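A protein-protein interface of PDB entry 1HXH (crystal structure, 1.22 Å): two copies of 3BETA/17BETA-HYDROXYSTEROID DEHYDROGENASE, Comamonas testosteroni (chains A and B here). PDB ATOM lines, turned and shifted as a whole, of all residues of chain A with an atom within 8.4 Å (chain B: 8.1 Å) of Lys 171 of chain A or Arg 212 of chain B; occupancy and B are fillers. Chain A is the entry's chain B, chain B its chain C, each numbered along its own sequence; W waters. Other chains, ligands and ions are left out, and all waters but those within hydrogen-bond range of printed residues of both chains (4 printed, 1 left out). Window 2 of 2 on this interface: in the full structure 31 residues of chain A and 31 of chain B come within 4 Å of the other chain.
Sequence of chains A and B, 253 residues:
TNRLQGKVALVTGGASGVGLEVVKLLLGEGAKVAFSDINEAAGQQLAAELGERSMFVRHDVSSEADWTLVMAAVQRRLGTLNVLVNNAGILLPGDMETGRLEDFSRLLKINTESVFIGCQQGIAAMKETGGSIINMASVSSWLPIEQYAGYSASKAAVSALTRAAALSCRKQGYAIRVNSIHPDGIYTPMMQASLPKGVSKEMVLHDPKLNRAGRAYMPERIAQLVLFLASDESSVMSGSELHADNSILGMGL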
ATOM      1  N   ALA A 164     -24.087 -15.553  12.357  1.00  0.00           N
ATOM      2  CA  ALA A 164     -25.096 -16.430  11.794  1.00  0.00           C
ATOM      3  C   ALA A 164     -24.843 -16.648  10.303  1.00  0.00           C
ATOM      4  O   ALA A 164     -24.950 -17.760   9.778  1.00  0.00           O
ATOM      5  CB  ALA A 164     -26.476 -15.847  11.978  1.00  0.00           C
ATOM      6  N   ALA A 165     -24.508 -15.585   9.564  1.00  0.00           N
ATOM      7  CA  ALA A 165     -24.252 -15.706   8.138  1.00  0.00           C
ATOM      8  C   ALA A 165     -23.013 -16.556   7.883  1.00  0.00           C
ATOM      9  O   ALA A 165     -23.016 -17.408   7.015  1.00  0.00           O
ATOM     10  CB  ALA A 165     -24.109 -14.321   7.508  1.00  0.00           C
ATOM     11  N   ALA A 166     -21.956 -16.315   8.654  1.00  0.00           N
ATOM     12  CA  ALA A 166     -20.732 -17.091   8.479  1.00  0.00           C
ATOM     13  C   ALA A 166     -20.983 -18.594   8.734  1.00  0.00           C
ATOM     14  O   ALA A 166     -20.484 -19.435   7.969  1.00  0.00           O
ATOM     15  CB  ALA A 166     -19.669 -16.548   9.415  1.00  0.00           C
ATOM     16  N   LEU A 167     -21.755 -18.884   9.767  1.00  0.00           N
ATOM     17  CA  LEU A 167     -22.040 -20.281  10.132  1.00  0.00           C
ATOM     18  C   LEU A 167     -22.866 -20.955   9.070  1.00  0.00           C
ATOM     19  O   LEU A 167     -22.569 -22.062   8.679  1.00  0.00           O
ATOM     20  CB  LEU A 167     -22.726 -20.345  11.496  1.00  0.00           C
ATOM     21  CG  LEU A 167     -23.016 -21.750  11.975  1.00  0.00           C
ATOM     22  CD1 LEU A 167     -21.724 -22.560  12.148  1.00  0.00           C
ATOM     23  CD2 LEU A 167     -23.821 -21.703  13.238  1.00  0.00           C
ATOM     24  N   SER A 168     -23.895 -20.257   8.599  1.00  0.00           N
ATOM     25  CA  SER A 168     -24.709 -20.877   7.527  1.00  0.00           C
ATOM     26  C   SER A 168     -23.866 -21.127   6.307  1.00  0.00           C
ATOM     27  O   SER A 168     -23.966 -22.173   5.658  1.00  0.00           O
ATOM     28  CB  SER A 168     -25.826 -19.910   7.173  1.00  0.00           C
ATOM     29  OG  SER A 168     -26.847 -19.991   8.100  1.00  0.00           O
ATOM     30  N   CYS A 169     -22.983 -20.187   5.959  1.00  0.00           N
ATOM     31  CA  CYS A 169     -22.146 -20.389   4.784  1.00  0.00           C
ATOM     32  C   CYS A 169     -21.265 -21.633   5.020  1.00  0.00           C
ATOM     33  O   CYS A 169     -21.097 -22.422   4.095  1.00  0.00           O
ATOM     34  CB  CYS A 169     -21.301 -19.163   4.442  1.00  0.00           C
ATOM     35  SG  CYS A 169     -22.312 -17.806   3.789  1.00  0.00           S
ATOM     36  N   ARG A 170     -20.658 -21.773   6.186  1.00  0.00           N
ATOM     37  CA  ARG A 170     -19.811 -22.947   6.404  1.00  0.00           C
ATOM     38  C   ARG A 170     -20.644 -24.243   6.319  1.00  0.00           C
ATOM     39  O   ARG A 170     -20.221 -25.213   5.679  1.00  0.00           O
ATOM     40  CB  ARG A 170     -19.107 -22.842   7.749  1.00  0.00           C
ATOM     41  CG  ARG A 170     -18.196 -24.046   7.922  1.00  0.00           C
ATOM     42  CD  ARG A 170     -17.262 -23.920   9.094  1.00  0.00           C
ATOM     43  NE  ARG A 170     -16.561 -25.195   9.268  1.00  0.00           N
ATOM     44  CZ  ARG A 170     -15.497 -25.371   9.999  1.00  0.00           C
ATOM     45  NH1 ARG A 170     -14.962 -24.364  10.659  1.00  0.00           N
ATOM     46  NH2 ARG A 170     -14.982 -26.562  10.097  1.00  0.00           N
ATOM     47  N   LYS A 171     -21.803 -24.273   6.967  1.00  0.00           N
ATOM     48  CA  LYS A 171     -22.619 -25.481   7.020  1.00  0.00           C
ATOM     49  C   LYS A 171     -23.147 -25.878   5.656  1.00  0.00           C
ATOM     50  O   LYS A 171     -23.293 -27.082   5.394  1.00  0.00           O
ATOM     51  CB  LYS A 171     -23.776 -25.343   8.029  1.00  0.00           C
ATOM     52  CG  LYS A 171     -23.346 -25.344   9.476  1.00  0.00           C
ATOM     53  CD  LYS A 171     -24.435 -25.200  10.460  1.00  0.00           C
ATOM     54  CE  LYS A 171     -25.181 -26.498  10.691  1.00  0.00           C
ATOM     55  NZ  LYS A 171     -26.395 -26.256  11.501  1.00  0.00           N
ATOM     56  N   GLN A 172     -23.402 -24.886   4.790  1.00  0.00           N
ATOM     57  CA  GLN A 172     -23.932 -25.117   3.458  1.00  0.00           C
ATOM     58  C   GLN A 172     -22.853 -25.284   2.411  1.00  0.00           C
ATOM     59  O   GLN A 172     -23.158 -25.552   1.254  1.00  0.00           O
ATOM     60  CB  GLN A 172     -24.882 -24.016   3.008  1.00  0.00           C
ATOM     61  CG  GLN A 172     -25.951 -23.619   4.028  1.00  0.00           C
ATOM     62  CD  GLN A 172     -26.789 -24.846   4.333  1.00  0.00           C
ATOM     63  OE1 GLN A 172     -26.814 -25.517   5.363  1.00  0.00           O
ATOM     64  NE2 GLN A 172     -27.512 -25.173   3.295  1.00  0.00           N
ATOM     65  N   GLY A 173     -21.578 -25.193   2.796  1.00  0.00           N
ATOM     66  CA  GLY A 173     -20.519 -25.368   1.794  1.00  0.00           C
ATOM     67  C   GLY A 173     -20.292 -24.246   0.821  1.00  0.00           C
ATOM     68  O   GLY A 173     -19.741 -24.441  -0.261  1.00  0.00           O
ATOM     69  N   TYR A 174     -20.704 -23.036   1.210  1.00  0.00           N
ATOM     70  CA  TYR A 174     -20.438 -21.847   0.408  1.00  0.00           C
ATOM     71  C   TYR A 174     -19.078 -21.279   0.775  1.00  0.00           C
ATOM     72  O   TYR A 174     -18.790 -21.122   1.961  1.00  0.00           O
ATOM     73  CB  TYR A 174     -21.493 -20.774   0.588  1.00  0.00           C
ATOM     74  CG  TYR A 174     -22.942 -21.236   0.466  1.00  0.00           C
ATOM     75  CD1 TYR A 174     -23.931 -20.545   1.155  1.00  0.00           C
ATOM     76  CD2 TYR A 174     -23.344 -22.301  -0.307  1.00  0.00           C
ATOM     77  CE1 TYR A 174     -25.251 -20.892   1.086  1.00  0.00           C
ATOM     78  CE2 TYR A 174     -24.689 -22.669  -0.381  1.00  0.00           C
ATOM     79  CZ  TYR A 174     -25.641 -21.963   0.324  1.00  0.00           C
ATOM     80  OH  TYR A 174     -26.962 -22.370   0.235  1.00  0.00           O
ATOM     81  N   ILE A 176     -17.887 -18.545   1.233  1.00  0.00           N
ATOM     82  CA  ILE A 176     -18.154 -17.166   1.570  1.00  0.00           C
ATOM     83  C   ILE A 176     -17.722 -16.925   3.016  1.00  0.00           C
ATOM     84  O   ILE A 176     -18.145 -17.684   3.897  1.00  0.00           O
ATOM     85  CB  ILE A 176     -19.640 -16.807   1.418  1.00  0.00           C
ATOM     86  CG1 ILE A 176     -20.178 -17.055   0.023  1.00  0.00           C
ATOM     87  CG2 ILE A 176     -19.877 -15.365   1.885  1.00  0.00           C
ATOM     88  CD1 ILE A 176     -21.686 -16.962  -0.084  1.00  0.00           C
ATOM     89  N   GLU B 202      -7.131 -34.964   2.786  1.00  0.00           N
ATOM     90  CA  GLU B 202      -8.492 -34.497   2.491  1.00  0.00           C
ATOM     91  C   GLU B 202      -9.451 -34.862   3.606  1.00  0.00           C
ATOM     92  O   GLU B 202     -10.487 -34.215   3.735  1.00  0.00           O
ATOM     93  CB  GLU B 202      -8.932 -35.049   1.143  1.00  0.00           C
ATOM     94  CG  GLU B 202      -8.099 -34.573  -0.027  1.00  0.00           C
ATOM     95  CD  GLU B 202      -6.641 -34.947  -0.176  1.00  0.00           C
ATOM     96  OE1 GLU B 202      -6.235 -36.074   0.280  1.00  0.00           O
ATOM     97  OE2 GLU B 202      -5.923 -34.101  -0.791  1.00  0.00           O
ATOM     98  N   LEU B 205      -8.272 -31.676   6.356  1.00  0.00           N
ATOM     99  CA  LEU B 205      -8.368 -30.250   6.033  1.00  0.00           C
ATOM    100  C   LEU B 205      -9.809 -29.854   5.852  1.00  0.00           C
ATOM    101  O   LEU B 205     -10.602 -30.511   5.179  1.00  0.00           O
ATOM    102  CB  LEU B 205      -7.699 -30.003   4.699  1.00  0.00           C
ATOM    103  CG  LEU B 205      -6.251 -29.763   4.498  1.00  0.00           C
ATOM    104  CD1 LEU B 205      -6.114 -29.296   3.033  1.00  0.00           C
ATOM    105  CD2 LEU B 205      -5.611 -28.752   5.419  1.00  0.00           C
ATOM    106  N   HIS B 206     -10.181 -28.670   6.355  1.00  0.00           N
ATOM    107  CA  HIS B 206     -11.469 -28.095   5.966  1.00  0.00           C
ATOM    108  C   HIS B 206     -11.567 -27.915   4.453  1.00  0.00           C
ATOM    109  O   HIS B 206     -10.607 -27.465   3.790  1.00  0.00           O
ATOM    110  CB  HIS B 206     -11.715 -26.752   6.631  1.00  0.00           C
ATOM    111  CG  HIS B 206     -12.917 -26.105   6.061  1.00  0.00           C
ATOM    112  ND1 HIS B 206     -12.899 -25.201   5.058  1.00  0.00           N
ATOM    113  CD2 HIS B 206     -14.232 -26.309   6.380  1.00  0.00           C
ATOM    114  CE1 HIS B 206     -14.136 -24.877   4.742  1.00  0.00           C
ATOM    115  NE2 HIS B 206     -14.981 -25.514   5.533  1.00  0.00           N
ATOM    116  N   ASP B 207     -12.707 -28.250   3.861  1.00  0.00           N
ATOM    117  CA  ASP B 207     -12.987 -27.975   2.473  1.00  0.00           C
ATOM    118  C   ASP B 207     -14.494 -27.827   2.342  1.00  0.00           C
ATOM    119  O   ASP B 207     -15.216 -28.651   2.898  1.00  0.00           O
ATOM    120  CB  ASP B 207     -12.483 -29.123   1.580  1.00  0.00           C
ATOM    121  CG  ASP B 207     -12.719 -28.755   0.125  1.00  0.00           C
ATOM    122  OD1 ASP B 207     -13.788 -29.007  -0.410  1.00  0.00           O
ATOM    123  OD2 ASP B 207     -11.821 -28.094  -0.471  1.00  0.00           O
ATOM    124  N   PRO B 208     -15.014 -26.791   1.698  1.00  0.00           N
ATOM    125  CA  PRO B 208     -16.471 -26.584   1.651  1.00  0.00           C
ATOM    126  C   PRO B 208     -17.246 -27.656   0.886  1.00  0.00           C
ATOM    127  O   PRO B 208     -18.427 -27.871   1.152  1.00  0.00           O
ATOM    128  CB  PRO B 208     -16.626 -25.220   0.973  1.00  0.00           C
ATOM    129  CG  PRO B 208     -15.376 -25.051   0.157  1.00  0.00           C
ATOM    130  CD  PRO B 208     -14.312 -25.690   1.010  1.00  0.00           C
ATOM    131  N   LYS B 209     -16.557 -28.330  -0.033  1.00  0.00           N
ATOM    132  CA  LYS B 209     -17.194 -29.399  -0.802  1.00  0.00           C
ATOM    133  C   LYS B 209     -16.959 -30.761  -0.195  1.00  0.00           C
ATOM    134  O   LYS B 209     -17.923 -31.520  -0.187  1.00  0.00           O
ATOM    135  CB  LYS B 209     -16.643 -29.320  -2.250  1.00  0.00           C
ATOM    136  CG  LYS B 209     -17.411 -30.203  -3.187  1.00  0.00           C
ATOM    137  CD  LYS B 209     -17.312 -29.737  -4.637  1.00  0.00           C
ATOM    138  CE  LYS B 209     -18.485 -28.871  -5.075  1.00  0.00           C
ATOM    139  NZ  LYS B 209     -19.815 -29.557  -4.992  1.00  0.00           N
ATOM    140  N   LEU B 210     -15.766 -31.057   0.297  1.00  0.00           N
ATOM    141  CA  LEU B 210     -15.370 -32.361   0.751  1.00  0.00           C
ATOM    142  C   LEU B 210     -15.339 -32.576   2.265  1.00  0.00           C
ATOM    143  O   LEU B 210     -15.368 -33.742   2.702  1.00  0.00           O
ATOM    144  CB  LEU B 210     -13.967 -32.721   0.277  1.00  0.00           C
ATOM    145  CG  LEU B 210     -13.733 -32.632  -1.212  1.00  0.00           C
ATOM    146  CD1 LEU B 210     -12.316 -32.987  -1.578  1.00  0.00           C
ATOM    147  CD2 LEU B 210     -14.721 -33.569  -1.892  1.00  0.00           C
ATOM    148  N   ASN B 211     -15.232 -31.557   3.077  1.00  0.00           N
ATOM    149  CA  ASN B 211     -15.067 -31.756   4.499  1.00  0.00           C
ATOM    150  C   ASN B 211     -15.428 -30.508   5.270  1.00  0.00           C
ATOM    151  O   ASN B 211     -14.515 -29.783   5.769  1.00  0.00           O
ATOM    152  CB  ASN B 211     -13.657 -32.200   4.799  1.00  0.00           C
ATOM    153  CG  ASN B 211     -13.364 -32.674   6.172  1.00  0.00           C
ATOM    154  OD1 ASN B 211     -12.153 -32.853   6.501  1.00  0.00           O
ATOM    155  ND2 ASN B 211     -14.340 -32.814   7.008  1.00  0.00           N
ATOM    156  N   ARG B 212     -16.687 -30.209   5.369  1.00  0.00           N
ATOM    157  CA  ARG B 212     -17.134 -28.979   6.017  1.00  0.00           C
ATOM    158  C   ARG B 212     -16.822 -28.954   7.502  1.00  0.00           C
ATOM    159  O   ARG B 212     -16.680 -27.873   8.077  1.00  0.00           O
ATOM    160  CB  ARG B 212     -18.632 -28.753   5.799  1.00  0.00           C
ATOM    161  CG  ARG B 212     -18.979 -28.592   4.331  1.00  0.00           C
ATOM    162  CD  ARG B 212     -20.471 -28.436   4.110  1.00  0.00           C
ATOM    163  NE  ARG B 212     -20.738 -28.581   2.705  1.00  0.00           N
ATOM    164  CZ  ARG B 212     -21.965 -28.625   2.175  1.00  0.00           C
ATOM    165  NH1 ARG B 212     -23.020 -28.482   2.947  1.00  0.00           N
ATOM    166  NH2 ARG B 212     -22.057 -28.786   0.864  1.00  0.00           N
ATOM    167  N   ALA B 213     -16.716 -30.105   8.144  1.00  0.00           N
ATOM    168  CA  ALA B 213     -16.389 -30.184   9.552  1.00  0.00           C
ATOM    169  C   ALA B 213     -14.896 -30.226   9.836  1.00  0.00           C
ATOM    170  O   ALA B 213     -14.451 -30.309  11.012  1.00  0.00           O
ATOM    171  CB  ALA B 213     -17.016 -31.461  10.141  1.00  0.00           C
ATOM    172  N   GLY B 214     -14.071 -30.173   8.791  1.00  0.00           N
ATOM    173  CA  GLY B 214     -12.640 -30.235   9.015  1.00  0.00           C
ATOM    174  C   GLY B 214     -12.090 -29.091   9.870  1.00  0.00           C
ATOM    175  O   GLY B 214     -12.580 -27.968   9.758  1.00  0.00           O
ATOM    176  N   ARG B 215     -11.066 -29.385  10.619  1.00  0.00           N
ATOM    177  CA  ARG B 215     -10.516 -28.526  11.642  1.00  0.00           C
ATOM    178  C   ARG B 215      -9.136 -27.995  11.243  1.00  0.00           C
ATOM    179  O   ARG B 215      -8.568 -27.208  11.975  1.00  0.00           O
ATOM    180  CB  ARG B 215     -10.463 -29.234  12.993  1.00  0.00           C
ATOM    181  CG  ARG B 215     -11.726 -29.771  13.599  1.00  0.00           C
ATOM    182  CD  ARG B 215     -12.688 -28.672  13.945  1.00  0.00           C
ATOM    183  NE  ARG B 215     -12.139 -27.770  14.964  1.00  0.00           N
ATOM    184  CZ  ARG B 215     -12.225 -27.897  16.260  1.00  0.00           C
ATOM    185  NH1 ARG B 215     -12.920 -28.906  16.819  1.00  0.00           N
ATOM    186  NH2 ARG B 215     -11.635 -27.022  17.043  1.00  0.00           N
ATOM    187  N   TYR B 217      -6.034 -26.403   8.549  1.00  0.00           N
ATOM    188  CA  TYR B 217      -5.793 -25.372   7.553  1.00  0.00           C
ATOM    189  C   TYR B 217      -4.327 -25.362   7.158  1.00  0.00           C
ATOM    190  O   TYR B 217      -3.474 -25.640   7.986  1.00  0.00           O
ATOM    191  CB  TYR B 217      -6.262 -23.922   8.049  1.00  0.00           C
ATOM    192  CG  TYR B 217      -7.718 -24.027   8.377  1.00  0.00           C
ATOM    193  CD1 TYR B 217      -8.160 -24.500   9.620  1.00  0.00           C
ATOM    194  CD2 TYR B 217      -8.697 -23.737   7.440  1.00  0.00           C
ATOM    195  CE1 TYR B 217      -9.516 -24.638   9.882  1.00  0.00           C
ATOM    196  CE2 TYR B 217     -10.055 -23.882   7.686  1.00  0.00           C
ATOM    197  CZ  TYR B 217     -10.448 -24.324   8.931  1.00  0.00           C
ATOM    198  OH  TYR B 217     -11.785 -24.497   9.193  1.00  0.00           O
ATOM    199  N   ASN B 246     -12.272 -19.946  10.764  1.00  0.00           N
ATOM    200  CA  ASN B 246     -13.258 -20.218   9.735  1.00  0.00           C
ATOM    201  C   ASN B 246     -14.621 -20.607  10.295  1.00  0.00           C
ATOM    202  O   ASN B 246     -15.189 -21.650   9.960  1.00  0.00           O
ATOM    203  CB  ASN B 246     -12.679 -21.316   8.835  1.00  0.00           C
ATOM    204  CG  ASN B 246     -13.584 -21.710   7.701  1.00  0.00           C
ATOM    205  OD1 ASN B 246     -14.243 -20.831   7.121  1.00  0.00           O
ATOM    206  ND2 ASN B 246     -13.668 -23.010   7.432  1.00  0.00           N
ATOM    207  N   SER B 247     -15.153 -19.815  11.203  1.00  0.00           N
ATOM    208  CA  SER B 247     -16.488 -19.999  11.717  1.00  0.00           C
ATOM    209  C   SER B 247     -16.699 -21.340  12.406  1.00  0.00           C
ATOM    210  O   SER B 247     -17.725 -21.955  12.242  1.00  0.00           O
ATOM    211  CB  SER B 247     -17.530 -19.783  10.621  1.00  0.00           C
ATOM    212  OG  SER B 247     -18.849 -19.829  11.149  1.00  0.00           O
ATOM    213  N   ILE B 248     -15.755 -21.789  13.241  1.00  0.00           N
ATOM    214  CA  ILE B 248     -15.990 -23.030  13.985  1.00  0.00           C
ATOM    215  C   ILE B 248     -17.086 -22.876  15.003  1.00  0.00           C
ATOM    216  O   ILE B 248     -17.768 -23.828  15.359  1.00  0.00           O
ATOM    217  CB  ILE B 248     -14.669 -23.486  14.628  1.00  0.00           C
ATOM    218  CG1 ILE B 248     -14.760 -24.919  15.154  1.00  0.00           C
ATOM    219  CG2 ILE B 248     -14.196 -22.527  15.681  1.00  0.00           C
ATOM    220  CD1 ILE B 248     -15.023 -25.957  14.063  1.00  0.00           C
ATOM    221  N   LEU B 249     -17.265 -21.683  15.532  1.00  0.00           N
ATOM    222  CA  LEU B 249     -18.233 -21.501  16.603  1.00  0.00           C
ATOM    223  C   LEU B 249     -19.638 -21.744  16.120  1.00  0.00           C
ATOM    224  O   LEU B 249     -20.121 -21.101  15.186  1.00  0.00           O
ATOM    225  CB  LEU B 249     -18.127 -20.111  17.204  1.00  0.00           C
ATOM    226  CG  LEU B 249     -19.073 -19.868  18.382  1.00  0.00           C
ATOM    227  CD1 LEU B 249     -18.792 -20.774  19.555  1.00  0.00           C
ATOM    228  CD2 LEU B 249     -19.005 -18.383  18.769  1.00  0.00           C
ATOM    229  N   GLY B 250     -20.338 -22.665  16.736  1.00  0.00           N
ATOM    230  CA  GLY B 250     -21.653 -23.061  16.332  1.00  0.00           C
ATOM    231  C   GLY B 250     -21.682 -24.344  15.521  1.00  0.00           C
ATOM    232  O   GLY B 250     -22.758 -24.910  15.394  1.00  0.00           O
ATOM    233  N   MET B 251     -20.547 -24.780  15.033  1.00  0.00           N
ATOM    234  CA  MET B 251     -20.466 -26.063  14.340  1.00  0.00           C
ATOM    235  C   MET B 251     -20.668 -27.228  15.328  1.00  0.00           C
ATOM    236  O   MET B 251     -20.355 -27.059  16.510  1.00  0.00           O
ATOM    237  CB  MET B 251     -19.094 -26.226  13.691  1.00  0.00           C
ATOM    238  CG  MET B 251     -18.860 -25.327  12.505  1.00  0.00           C
ATOM    239  SD  MET B 251     -19.986 -25.618  11.096  1.00  0.00           S
ATOM    240  CE  MET B 251     -19.417 -27.217  10.549  1.00  0.00           C
ATOM    241  N   GLY B 252     -21.164 -28.358  14.828  1.00  0.00           N
ATOM    242  CA  GLY B 252     -21.261 -29.537  15.627  1.00  0.00           C
ATOM    243  C   GLY B 252     -22.510 -29.634  16.474  1.00  0.00           C
ATOM    244  O   GLY B 252     -22.739 -30.666  17.109  1.00  0.00           O
ATOM    245  N   LEU B 253     -23.305 -28.576  16.464  1.00  0.00           N
ATOM    246  CA  LEU B 253     -24.496 -28.449  17.289  1.00  0.00           C
ATOM    247  C   LEU B 253     -25.741 -28.478  16.418  1.00  0.00           C
ATOM    248  O   LEU B 253     -26.822 -28.845  17.067  1.00  0.00           O
ATOM    249  CB  LEU B 253     -24.418 -27.135  18.064  1.00  0.00           C
ATOM    250  CG  LEU B 253     -23.270 -26.991  19.087  1.00  0.00           C
ATOM    251  CD1 LEU B 253     -23.311 -25.568  19.570  1.00  0.00           C
ATOM    252  CD2 LEU B 253     -23.425 -27.981  20.228  1.00  0.00           C
ATOM    253  OXT LEU B 253     -25.728 -28.200  15.277  1.00  0.00           O
HETATM  254  O   HOH W   1     -24.109 -26.769  13.909  1.00  0.00           O
HETATM  255  O   HOH W   2     -12.306 -24.490  11.794  1.00  0.00           O
HETATM  256  O   HOH W   3     -26.100 -28.052   4.022  1.00  0.00           O
HETATM  257  O   HOH W   4     -17.673 -25.220   4.531  1.00  0.00           O
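Hydrophobic or aromatic side chains of chain A that line the printed part of chain B: Ala 166 and Leu 167. Among the printed residues, no Asp or Glu carboxylate lies within 4 Å of a Lys or Arg side-chain nitrogen of the other chain.
No position is printed for both chains.
The side-chain amide nitrogen (ND2) of Asn 246 of chain B lies close to a ring nitrogen (ND1) of His 206 of chain B (3.3 Å). O of Asp 207 of chain B is in hydrogen-bond range of N of Arg 212 of chain B (3.3 Å). NE of Arg 212 of chain B lies within hydrogen-bond range of O of Pro 208 of chain B, at 2.9 Å. The side-chain amide nitrogen (ND2) of Asn 211 of chain B sits close to the backbone NH (N) of Gly 214 of chain B (3.2 Å). The side-chain amide nitrogen (ND2) of Asn 246 of chain B lies within hydrogen-bond range of the side-chain hydroxyl (OH) of Tyr 217 of chain B (3.0 Å).
Of the printed residues of chain B, Leu 167 of chain A touches Ser 247, Leu 249, Gly 250 and Met 251. Lys 171 of chain A touches just these residues of chain B: Arg 212 and Met 251. Ile 176 of chain A touches none of the printed residues of chain B. Printed residues of chain A within 4 Å of Arg 212 of chain B: Arg 170 (2.9 Å), Lys 171 (2.8 Å), Gln 172 (3.2 Å) and Gly 173 (3.3 Å). Of the printed residues of chain A, Gly 214 of chain B touches Arg 170. Of the printed residues of chain A, Leu 249 of chain B touches Leu 167. Printed residues of chain A within 4 Å of Gly 250 of chain B: Leu 167. The nearest residue of chain B that does not touch Lys 171 of chain A is Leu 253 of chain B (4.3 Å). The nearest printed residue of chain A that does not touch Gly 250 of chain B is Lys 171 of chain A (5.2 Å).
Among the printed residues, pairs that only touch across the chains: Ala 166 of chain A with Ser 247 of chain B, Leu 167 of chain A with Leu 249 of chain B, Leu 167 of chain A with Gly 250 of chain B, Leu 167 of chain A with Met 251 of chain B, Arg 170 of chain A with His 206 of chain B, Arg 170 of chain A with Ala 213 of chain B, Arg 170 of chain A with Tyr 217 of chain B, Arg 170 of chain A with Ser 247 of chain B, Arg 170 of chain A with Ile 248 of chain B, Arg 170 of chain A with Met 251 of chain B, Lys 171 of chain A with Met 251 of chain B and Gly 173 of chain A with Pro 208 of chain B.
Water W1 lies within hydrogen-bond range of the chain-end carboxylate of Leu 253 of chain B, the backbone carbonyl oxygen of Gly 250 of chain B, the side-chain amino group of Lys 171 of chain A and the backbone NH of Gly 252 of chain B. Water W2 bridges OH of Tyr 217 of chain B (2.7 Å) and NH1 of Arg 170 of chain A (2.9 Å). Water W4 bridges O of Arg 170 of chain A (2.8 Å) and NE2 of His 206 of chain B (2.9 Å). Water W3 lies within hydrogen-bond range of OE1 of Gln 172 of chain A (3.0 Å), O of Lys 171 of chain A (3.3 Å) and NH1 of Arg 212 of chain B (3.3 Å).
The backbone NH (N) of Leu 167 of chain A is in hydrogen-bond range of the side-chain hydroxyl (OG) of Ser 247 of chain B (3.4 Å). The backbone carbonyl oxygen of Arg 212 of chain B sits at hydrogen-bond distance from the guanidinium group of Arg 170 of chain A (2.9 Å). The guanidinium group of Arg 170 of chain A sits at hydrogen-bond distance from the backbone carbonyl oxygen of Gly 214 of chain B (2.8 Å). The backbone carbonyl oxygen (O) of Asn 246 of chain B is in hydrogen-bond range of the guanidinium group (NH1) of Arg 170 of chain A (2.8 Å). The guanidinium group (NH1) of Arg 212 of chain B is in hydrogen-bond range of the backbone carbonyl oxygen (O) of Lys 171 of chain A, 2.8 Å away. NH1 of Arg 212 of chain B lies close to O of Gln 172 of chain A (3.4 Å). The backbone NH (N) of Gly 173 of chain A lies close to the guanidinium group (NE) of Arg 212 of chain B (3.5 Å).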
